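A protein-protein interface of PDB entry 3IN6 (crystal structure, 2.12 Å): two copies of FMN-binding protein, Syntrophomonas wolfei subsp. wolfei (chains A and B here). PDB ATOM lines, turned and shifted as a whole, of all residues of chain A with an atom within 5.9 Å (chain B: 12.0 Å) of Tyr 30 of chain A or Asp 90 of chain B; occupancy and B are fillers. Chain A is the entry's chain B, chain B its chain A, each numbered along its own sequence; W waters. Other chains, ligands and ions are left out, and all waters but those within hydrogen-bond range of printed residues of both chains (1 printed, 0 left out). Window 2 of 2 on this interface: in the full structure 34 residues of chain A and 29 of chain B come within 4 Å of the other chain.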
ATOM      1  N   SER A  24       8.213  -7.700  -7.421  1.00  0.00           N
ATOM      2  CA  SER A  24       8.353  -8.266  -8.764  1.00  0.00           C
ATOM      3  C   SER A  24       7.660  -9.617  -8.904  1.00  0.00           C
ATOM      4  O   SER A  24       7.044  -9.896  -9.937  1.00  0.00           O
ATOM      5  CB  SER A  24       9.823  -8.463  -9.122  1.00  0.00           C
ATOM      6  OG  SER A  24      10.518  -7.230  -9.159  1.00  0.00           O
ATOM      7  N   LEU A  25       7.754 -10.459  -7.875  1.00  0.00           N
ATOM      8  CA  LEU A  25       7.180 -11.807  -7.962  1.00  0.00           C
ATOM      9  C   LEU A  25       5.666 -11.785  -7.924  1.00  0.00           C
ATOM     10  O   LEU A  25       5.026 -12.475  -8.704  1.00  0.00           O
ATOM     11  CB  LEU A  25       7.744 -12.706  -6.868  1.00  0.00           C
ATOM     12  CG  LEU A  25       9.224 -13.054  -6.994  1.00  0.00           C
ATOM     13  CD1 LEU A  25       9.753 -13.656  -5.700  1.00  0.00           C
ATOM     14  CD2 LEU A  25       9.441 -13.991  -8.144  1.00  0.00           C
ATOM     15  N   ILE A  26       5.098 -10.988  -7.025  1.00  0.00           N
ATOM     16  CA  ILE A  26       3.646 -10.883  -6.885  1.00  0.00           C
ATOM     17  C   ILE A  26       2.997 -10.232  -8.090  1.00  0.00           C
ATOM     18  O   ILE A  26       2.026 -10.769  -8.638  1.00  0.00           O
ATOM     19  CB  ILE A  26       3.240 -10.090  -5.625  1.00  0.00           C
ATOM     20  CG1 ILE A  26       3.588 -10.866  -4.357  1.00  0.00           C
ATOM     21  CG2 ILE A  26       1.745  -9.782  -5.643  1.00  0.00           C
ATOM     22  CD1 ILE A  26       2.828 -12.191  -4.166  1.00  0.00           C
ATOM     23  N   ALA A  28       4.095 -10.095 -11.002  1.00  0.00           N
ATOM     24  CA  ALA A  28       4.351 -10.893 -12.208  1.00  0.00           C
ATOM     25  C   ALA A  28       3.182 -11.830 -12.492  1.00  0.00           C
ATOM     26  O   ALA A  28       2.979 -12.251 -13.633  1.00  0.00           O
ATOM     27  CB  ALA A  28       5.629 -11.684 -12.062  1.00  0.00           C
ATOM     28  N   ASN A  29       2.423 -12.159 -11.449  1.00  0.00           N
ATOM     29  CA  ASN A  29       1.245 -13.024 -11.562  1.00  0.00           C
ATOM     30  C   ASN A  29       1.534 -14.408 -12.136  1.00  0.00           C
ATOM     31  O   ASN A  29       0.845 -14.860 -13.046  1.00  0.00           O
ATOM     32  CB  ASN A  29       0.130 -12.344 -12.370  1.00  0.00           C
ATOM     33  CG  ASN A  29      -0.465 -11.138 -11.666  1.00  0.00           C
ATOM     34  OD1 ASN A  29      -1.335 -10.474 -12.215  1.00  0.00           O
ATOM     35  ND2 ASN A  29      -0.019 -10.861 -10.451  1.00  0.00           N
ATOM     36  N   TYR A  30       2.552 -15.079 -11.603  1.00  0.00           N
ATOM     37  CA  TYR A  30       2.859 -16.443 -12.039  1.00  0.00           C
ATOM     38  C   TYR A  30       1.691 -17.363 -11.699  1.00  0.00           C
ATOM     39  O   TYR A  30       1.001 -17.161 -10.696  1.00  0.00           O
ATOM     40  CB  TYR A  30       4.119 -16.981 -11.357  1.00  0.00           C
ATOM     41  CG  TYR A  30       5.390 -16.297 -11.776  1.00  0.00           C
ATOM     42  CD1 TYR A  30       6.056 -16.681 -12.934  1.00  0.00           C
ATOM     43  CD2 TYR A  30       5.932 -15.266 -11.018  1.00  0.00           C
ATOM     44  CE1 TYR A  30       7.224 -16.056 -13.328  1.00  0.00           C
ATOM     45  CE2 TYR A  30       7.105 -14.626 -11.411  1.00  0.00           C
ATOM     46  CZ  TYR A  30       7.746 -15.033 -12.560  1.00  0.00           C
ATOM     47  OH  TYR A  30       8.907 -14.417 -12.954  1.00  0.00           O
ATOM     48  N   ILE A  31       1.486 -18.385 -12.520  1.00  0.00           N
ATOM     49  CA  ILE A  31       0.413 -19.340 -12.271  1.00  0.00           C
ATOM     50  C   ILE A  31       0.758 -20.182 -11.048  1.00  0.00           C
ATOM     51  O   ILE A  31      -0.123 -20.767 -10.427  1.00  0.00           O
ATOM     52  CB  ILE A  31       0.147 -20.243 -13.491  1.00  0.00           C
ATOM     53  CG1 ILE A  31       1.284 -21.255 -13.683  1.00  0.00           C
ATOM     54  CG2 ILE A  31      -0.069 -19.389 -14.744  1.00  0.00           C
ATOM     55  CD1 ILE A  31       1.250 -21.972 -15.014  1.00  0.00           C
ATOM     56  N   SER A  32       2.045 -20.230 -10.703  1.00  0.00           N
ATOM     57  CA  SER A  32       2.511 -20.964  -9.539  1.00  0.00           C
ATOM     58  C   SER A  32       2.508 -20.050  -8.321  1.00  0.00           C
ATOM     59  O   SER A  32       3.531 -19.900  -7.653  1.00  0.00           O
ATOM     60  CB  SER A  32       3.915 -21.537  -9.787  1.00  0.00           C
ATOM     61  OG  SER A  32       4.865 -20.516 -10.085  1.00  0.00           O
ATOM     62  N   THR A  33       1.360 -19.428  -8.051  1.00  0.00           N
ATOM     63  CA  THR A  33       1.179 -18.545  -6.895  1.00  0.00           C
ATOM     64  C   THR A  33       0.001 -19.048  -6.087  1.00  0.00           C
ATOM     65  O   THR A  33      -1.095 -19.221  -6.618  1.00  0.00           O
ATOM     66  CB  THR A  33       0.921 -17.088  -7.316  1.00  0.00           C
ATOM     67  OG1 THR A  33       2.035 -16.621  -8.082  1.00  0.00           O
ATOM     68  CG2 THR A  33       0.745 -16.177  -6.083  1.00  0.00           C
ATOM     69  N   VAL A  48      -4.651 -21.992  -5.727  1.00  0.00           N
ATOM     70  CA  VAL A  48      -3.894 -21.181  -6.652  1.00  0.00           C
ATOM     71  C   VAL A  48      -4.633 -19.849  -6.836  1.00  0.00           C
ATOM     72  O   VAL A  48      -5.794 -19.822  -7.215  1.00  0.00           O
ATOM     73  CB  VAL A  48      -3.720 -21.882  -8.000  1.00  0.00           C
ATOM     74  CG1 VAL A  48      -2.995 -20.981  -8.970  1.00  0.00           C
ATOM     75  CG2 VAL A  48      -2.966 -23.199  -7.799  1.00  0.00           C
ATOM     76  N   ILE A  49      -3.945 -18.752  -6.538  1.00  0.00           N
ATOM     77  CA  ILE A  49      -4.492 -17.396  -6.665  1.00  0.00           C
ATOM     78  C   ILE A  49      -3.412 -16.520  -7.269  1.00  0.00           C
ATOM     79  O   ILE A  49      -2.412 -16.230  -6.602  1.00  0.00           O
ATOM     80  CB  ILE A  49      -4.902 -16.823  -5.295  1.00  0.00           C
ATOM     81  CG1 ILE A  49      -5.983 -17.703  -4.652  1.00  0.00           C
ATOM     82  CG2 ILE A  49      -5.389 -15.409  -5.451  1.00  0.00           C
ATOM     83  CD1 ILE A  49      -7.270 -17.878  -5.512  1.00  0.00           C
ATOM     84  N   SER A  50      -3.614 -16.109  -8.523  1.00  0.00           N
ATOM     85  CA  SER A  50      -2.616 -15.325  -9.257  1.00  0.00           C
ATOM     86  C   SER A  50      -3.027 -13.922  -9.735  1.00  0.00           C
ATOM     87  O   SER A  50      -2.156 -13.146 -10.118  1.00  0.00           O
ATOM     88  CB  SER A  50      -2.168 -16.117 -10.482  1.00  0.00           C
ATOM     89  OG  SER A  50      -3.237 -16.235 -11.396  1.00  0.00           O
ATOM     90  N   VAL A  84       5.050 -17.589  -4.016  1.00  0.00           N
ATOM     91  CA  VAL A  84       5.356 -17.636  -5.443  1.00  0.00           C
ATOM     92  C   VAL A  84       6.532 -18.601  -5.496  1.00  0.00           C
ATOM     93  O   VAL A  84       7.595 -18.303  -4.947  1.00  0.00           O
ATOM     94  CB  VAL A  84       5.745 -16.262  -6.020  1.00  0.00           C
ATOM     95  CG1 VAL A  84       6.090 -16.387  -7.514  1.00  0.00           C
ATOM     96  CG2 VAL A  84       4.620 -15.266  -5.813  1.00  0.00           C
ATOM     97  N   LEU A  86       9.054 -20.814  -7.854  1.00  0.00           N
ATOM     98  CA  LEU A  86       9.581 -21.001  -9.203  1.00  0.00           C
ATOM     99  C   LEU A  86      10.572 -22.151  -9.141  1.00  0.00           C
ATOM    100  O   LEU A  86      11.415 -22.183  -8.250  1.00  0.00           O
ATOM    101  CB  LEU A  86      10.281 -19.721  -9.664  1.00  0.00           C
ATOM    102  CG  LEU A  86       9.469 -18.417  -9.630  1.00  0.00           C
ATOM    103  CD1 LEU A  86      10.311 -17.235 -10.104  1.00  0.00           C
ATOM    104  CD2 LEU A  86       8.203 -18.518 -10.457  1.00  0.00           C
ATOM    105  N   SER B  32       8.441 -28.649  -6.436  1.00  0.00           N
ATOM    106  CA  SER B  32       7.243 -27.838  -6.301  1.00  0.00           C
ATOM    107  C   SER B  32       6.151 -28.552  -5.498  1.00  0.00           C
ATOM    108  O   SER B  32       5.045 -28.786  -5.993  1.00  0.00           O
ATOM    109  CB  SER B  32       6.733 -27.479  -7.692  1.00  0.00           C
ATOM    110  OG  SER B  32       6.139 -28.615  -8.268  1.00  0.00           O
ATOM    111  N   MET B  83       0.356 -29.742  -1.042  1.00  0.00           N
ATOM    112  CA  MET B  83      -0.019 -29.443  -2.389  1.00  0.00           C
ATOM    113  C   MET B  83       1.162 -29.701  -3.277  1.00  0.00           C
ATOM    114  O   MET B  83       2.282 -29.322  -2.946  1.00  0.00           O
ATOM    115  CB  MET B  83      -0.464 -27.994  -2.605  1.00  0.00           C
ATOM    116  CG  MET B  83      -0.747 -27.722  -4.136  1.00  0.00           C
ATOM    117  SD  MET B  83      -1.464 -26.011  -4.638  1.00  0.00           S
ATOM    118  CE  MET B  83      -3.356 -26.320  -4.524  1.00  0.00           C
ATOM    119  N   LEU B  85       2.123 -29.067  -7.367  1.00  0.00           N
ATOM    120  CA  LEU B  85       1.685 -28.233  -8.467  1.00  0.00           C
ATOM    121  C   LEU B  85       2.739 -28.268  -9.575  1.00  0.00           C
ATOM    122  O   LEU B  85       3.863 -27.830  -9.379  1.00  0.00           O
ATOM    123  CB  LEU B  85       1.528 -26.794  -7.981  1.00  0.00           C
ATOM    124  CG  LEU B  85       0.873 -25.806  -8.941  1.00  0.00           C
ATOM    125  CD1 LEU B  85      -0.563 -26.222  -9.211  1.00  0.00           C
ATOM    126  CD2 LEU B  85       0.923 -24.399  -8.360  1.00  0.00           C
ATOM    127  N   LEU B  86       2.394 -28.829 -10.712  1.00  0.00           N
ATOM    128  CA  LEU B  86       3.327 -28.863 -11.827  1.00  0.00           C
ATOM    129  C   LEU B  86       2.927 -27.777 -12.794  1.00  0.00           C
ATOM    130  O   LEU B  86       1.743 -27.616 -13.098  1.00  0.00           O
ATOM    131  CB  LEU B  86       3.339 -30.240 -12.498  1.00  0.00           C
ATOM    132  CG  LEU B  86       4.012 -31.339 -11.662  1.00  0.00           C
ATOM    133  CD1 LEU B  86       3.865 -32.708 -12.288  1.00  0.00           C
ATOM    134  CD2 LEU B  86       5.497 -31.030 -11.394  1.00  0.00           C
ATOM    135  N   THR B  87       3.919 -27.000 -13.219  1.00  0.00           N
ATOM    136  CA  THR B  87       3.751 -25.963 -14.230  1.00  0.00           C
ATOM    137  C   THR B  87       4.993 -26.034 -15.135  1.00  0.00           C
ATOM    138  O   THR B  87       6.118 -26.148 -14.645  1.00  0.00           O
ATOM    139  CB  THR B  87       3.596 -24.559 -13.604  1.00  0.00           C
ATOM    140  OG1 THR B  87       4.823 -24.164 -12.986  1.00  0.00           O
ATOM    141  CG2 THR B  87       2.488 -24.549 -12.552  1.00  0.00           C
ATOM    142  N   ASP B  88       4.793 -26.000 -16.447  1.00  0.00           N
ATOM    143  CA  ASP B  88       5.899 -26.087 -17.395  1.00  0.00           C
ATOM    144  C   ASP B  88       5.957 -24.794 -18.177  1.00  0.00           C
ATOM    145  O   ASP B  88       5.039 -24.493 -18.934  1.00  0.00           O
ATOM    146  N   ASN B  89       7.030 -24.028 -17.986  1.00  0.00           N
ATOM    147  CA  ASN B  89       7.196 -22.742 -18.668  1.00  0.00           C
ATOM    148  C   ASN B  89       5.972 -21.853 -18.449  1.00  0.00           C
ATOM    149  O   ASN B  89       5.410 -21.307 -19.399  1.00  0.00           O
ATOM    150  N   ASP B  90       5.575 -21.729 -17.187  1.00  0.00           N
ATOM    151  CA  ASP B  90       4.395 -20.966 -16.779  1.00  0.00           C
ATOM    152  C   ASP B  90       3.168 -21.398 -17.584  1.00  0.00           C
ATOM    153  O   ASP B  90       2.445 -20.581 -18.160  1.00  0.00           O
ATOM    154  CB  ASP B  90       4.630 -19.452 -16.876  1.00  0.00           C
ATOM    155  CG  ASP B  90       3.693 -18.650 -15.965  1.00  0.00           C
ATOM    156  OD1 ASP B  90       3.577 -18.992 -14.764  1.00  0.00           O
ATOM    157  OD2 ASP B  90       3.098 -17.659 -16.442  1.00  0.00           O
ATOM    158  N   LYS B  91       2.979 -22.711 -17.640  1.00  0.00           N
ATOM    159  CA  LYS B  91       1.819 -23.324 -18.265  1.00  0.00           C
ATOM    160  C   LYS B  91       1.388 -24.332 -17.219  1.00  0.00           C
ATOM    161  O   LYS B  91       2.230 -25.047 -16.681  1.00  0.00           O
ATOM    162  CB  LYS B  91       2.188 -24.043 -19.562  1.00  0.00           C
ATOM    163  CG  LYS B  91       0.990 -24.478 -20.401  1.00  0.00           C
ATOM    164  CD  LYS B  91       0.349 -23.314 -21.158  1.00  0.00           C
ATOM    165  CE  LYS B  91       1.185 -22.865 -22.351  1.00  0.00           C
ATOM    166  NZ  LYS B  91       1.283 -23.927 -23.392  1.00  0.00           N
ATOM    167  N   SER B  92       0.102 -24.369 -16.890  1.00  0.00           N
ATOM    168  CA  SER B  92      -0.377 -25.321 -15.892  1.00  0.00           C
ATOM    169  C   SER B  92      -0.281 -26.732 -16.472  1.00  0.00           C
ATOM    170  O   SER B  92      -0.662 -26.954 -17.631  1.00  0.00           O
ATOM    171  CB  SER B  92      -1.822 -25.017 -15.498  1.00  0.00           C
ATOM    172  OG  SER B  92      -2.337 -26.029 -14.654  1.00  0.00           O
ATOM    173  N   LYS B  93       0.263 -27.663 -15.689  1.00  0.00           N
ATOM    174  CA  LYS B  93       0.383 -29.065 -16.110  1.00  0.00           C
ATOM    175  C   LYS B  93      -0.516 -29.987 -15.321  1.00  0.00           C
ATOM    176  O   LYS B  93      -1.326 -30.697 -15.912  1.00  0.00           O
ATOM    177  CB  LYS B  93       1.835 -29.561 -16.046  1.00  0.00           C
ATOM    178  CG  LYS B  93       2.485 -29.803 -17.415  1.00  0.00           C
ATOM    179  CD  LYS B  93       2.438 -28.612 -18.340  1.00  0.00           C
ATOM    180  CE  LYS B  93       2.763 -29.048 -19.753  1.00  0.00           C
ATOM    181  NZ  LYS B  93       2.701 -27.919 -20.702  1.00  0.00           N
ATOM    182  N   ASP B  94      -0.376 -29.982 -13.993  1.00  0.00           N
ATOM    183  CA  ASP B  94      -1.169 -30.861 -13.143  1.00  0.00           C
ATOM    184  C   ASP B  94      -0.881 -30.582 -11.664  1.00  0.00           C
ATOM    185  O   ASP B  94      -0.027 -29.771 -11.332  1.00  0.00           O
ATOM    186  CB  ASP B  94      -0.815 -32.318 -13.452  1.00  0.00           C
ATOM    187  CG  ASP B  94      -1.893 -33.287 -13.026  1.00  0.00           C
ATOM    188  OD1 ASP B  94      -3.089 -32.980 -13.238  1.00  0.00           O
ATOM    189  OD2 ASP B  94      -1.541 -34.367 -12.505  1.00  0.00           O
ATOM    190  N   VAL B 143      -6.576 -29.630  -7.881  1.00  0.00           N
ATOM    191  CA  VAL B 143      -5.994 -28.292  -7.727  1.00  0.00           C
ATOM    192  C   VAL B 143      -7.020 -27.169  -7.654  1.00  0.00           C
ATOM    193  O   VAL B 143      -6.983 -26.377  -6.718  1.00  0.00           O
ATOM    194  CB  VAL B 143      -4.940 -28.001  -8.828  1.00  0.00           C
ATOM    195  CG1 VAL B 143      -4.757 -26.513  -9.036  1.00  0.00           C
ATOM    196  CG2 VAL B 143      -3.632 -28.665  -8.443  1.00  0.00           C
HETATM  197  O   HOH W   1      -6.542 -23.890  -6.533  1.00  0.00           O
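Tyr 30 of chain A touches one residue of chain B.
Asp 90 of chain B touches just these residues of chain A: Tyr 30 and Ile 31.
No residue of chain B comes within 4 Å of Leu 25 of chain A.
No residue of chain B comes within 4 Å of Asn 29 of chain A.
Ser 32 of chain A touches just one residue of chain B: Leu 85.
No residue of chain B comes within 4 Å of Thr 33 of chain A.
Of the printed residues of chain A, Thr 87 of chain B touches Ile 31 (3.7 Å).
Printed residues of chain A within 4 Å of Val 143 of chain B: Val 48 (3.96 Å).
Of the printed residues of chain A, Leu 85 of chain B touches Ser 32 (3.96 Å).
Of the printed residues of chain A, Lys 91 of chain B touches Ile 31.
Ile 26 of chain A touches none of the printed residues of chain B.
Ser 24 of chain A touches none of the printed residues of chain B.
The nearest residue of chain B that does not touch Tyr 30 of chain A is Thr 87 of chain B (7.3 Å).
Water W1 lies within hydrogen-bond range of the backbone carbonyl oxygen of Val 143 of chain B (2.5 Å) and the backbone NH of Val 48 of chain A (2.8 Å).
Of the 14 printed residues of chain A, 4 touch a printed residue of chain B.
Printed residues of chain B that touch a printed residue of chain A: Leu 85, Thr 87, Asp 90, Lys 91, Ser 92 and Val 143.
Hydrophobic or aromatic side chains of chain B that line the printed part of chain A: Leu 85 and Val 143.
Positions printed for both chains: 32 and 86.
OD1 of Asp 90 of chain B lies within hydrogen-bond range of N of Ile 31 of chain A, at 3.1 Å.
O of Leu 85 of chain B lies within hydrogen-bond range of OG of Ser 32 of chain B (2.7 Å).
O of Tyr 30 of chain A sits at hydrogen-bond distance from OG1 of Thr 33 of chain A (2.9 Å).
OD1 of Asp 90 of chain B touches CA of Tyr 30 of chain A, 3.8 Å away.
CG2 of Thr 87 of chain B touches CG1 of Ile 31 of chain A, 3.7 Å away.
N of Lys 91 of chain B touches CD1 of Ile 31 of chain A, at 3.2 Å.
Ser 92 of chain B touches Ile 31 of chain A.
Ser 32 of chain A touches Leu 85 of chain B.
Val 48 of chain A touches Val 143 of chain B.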
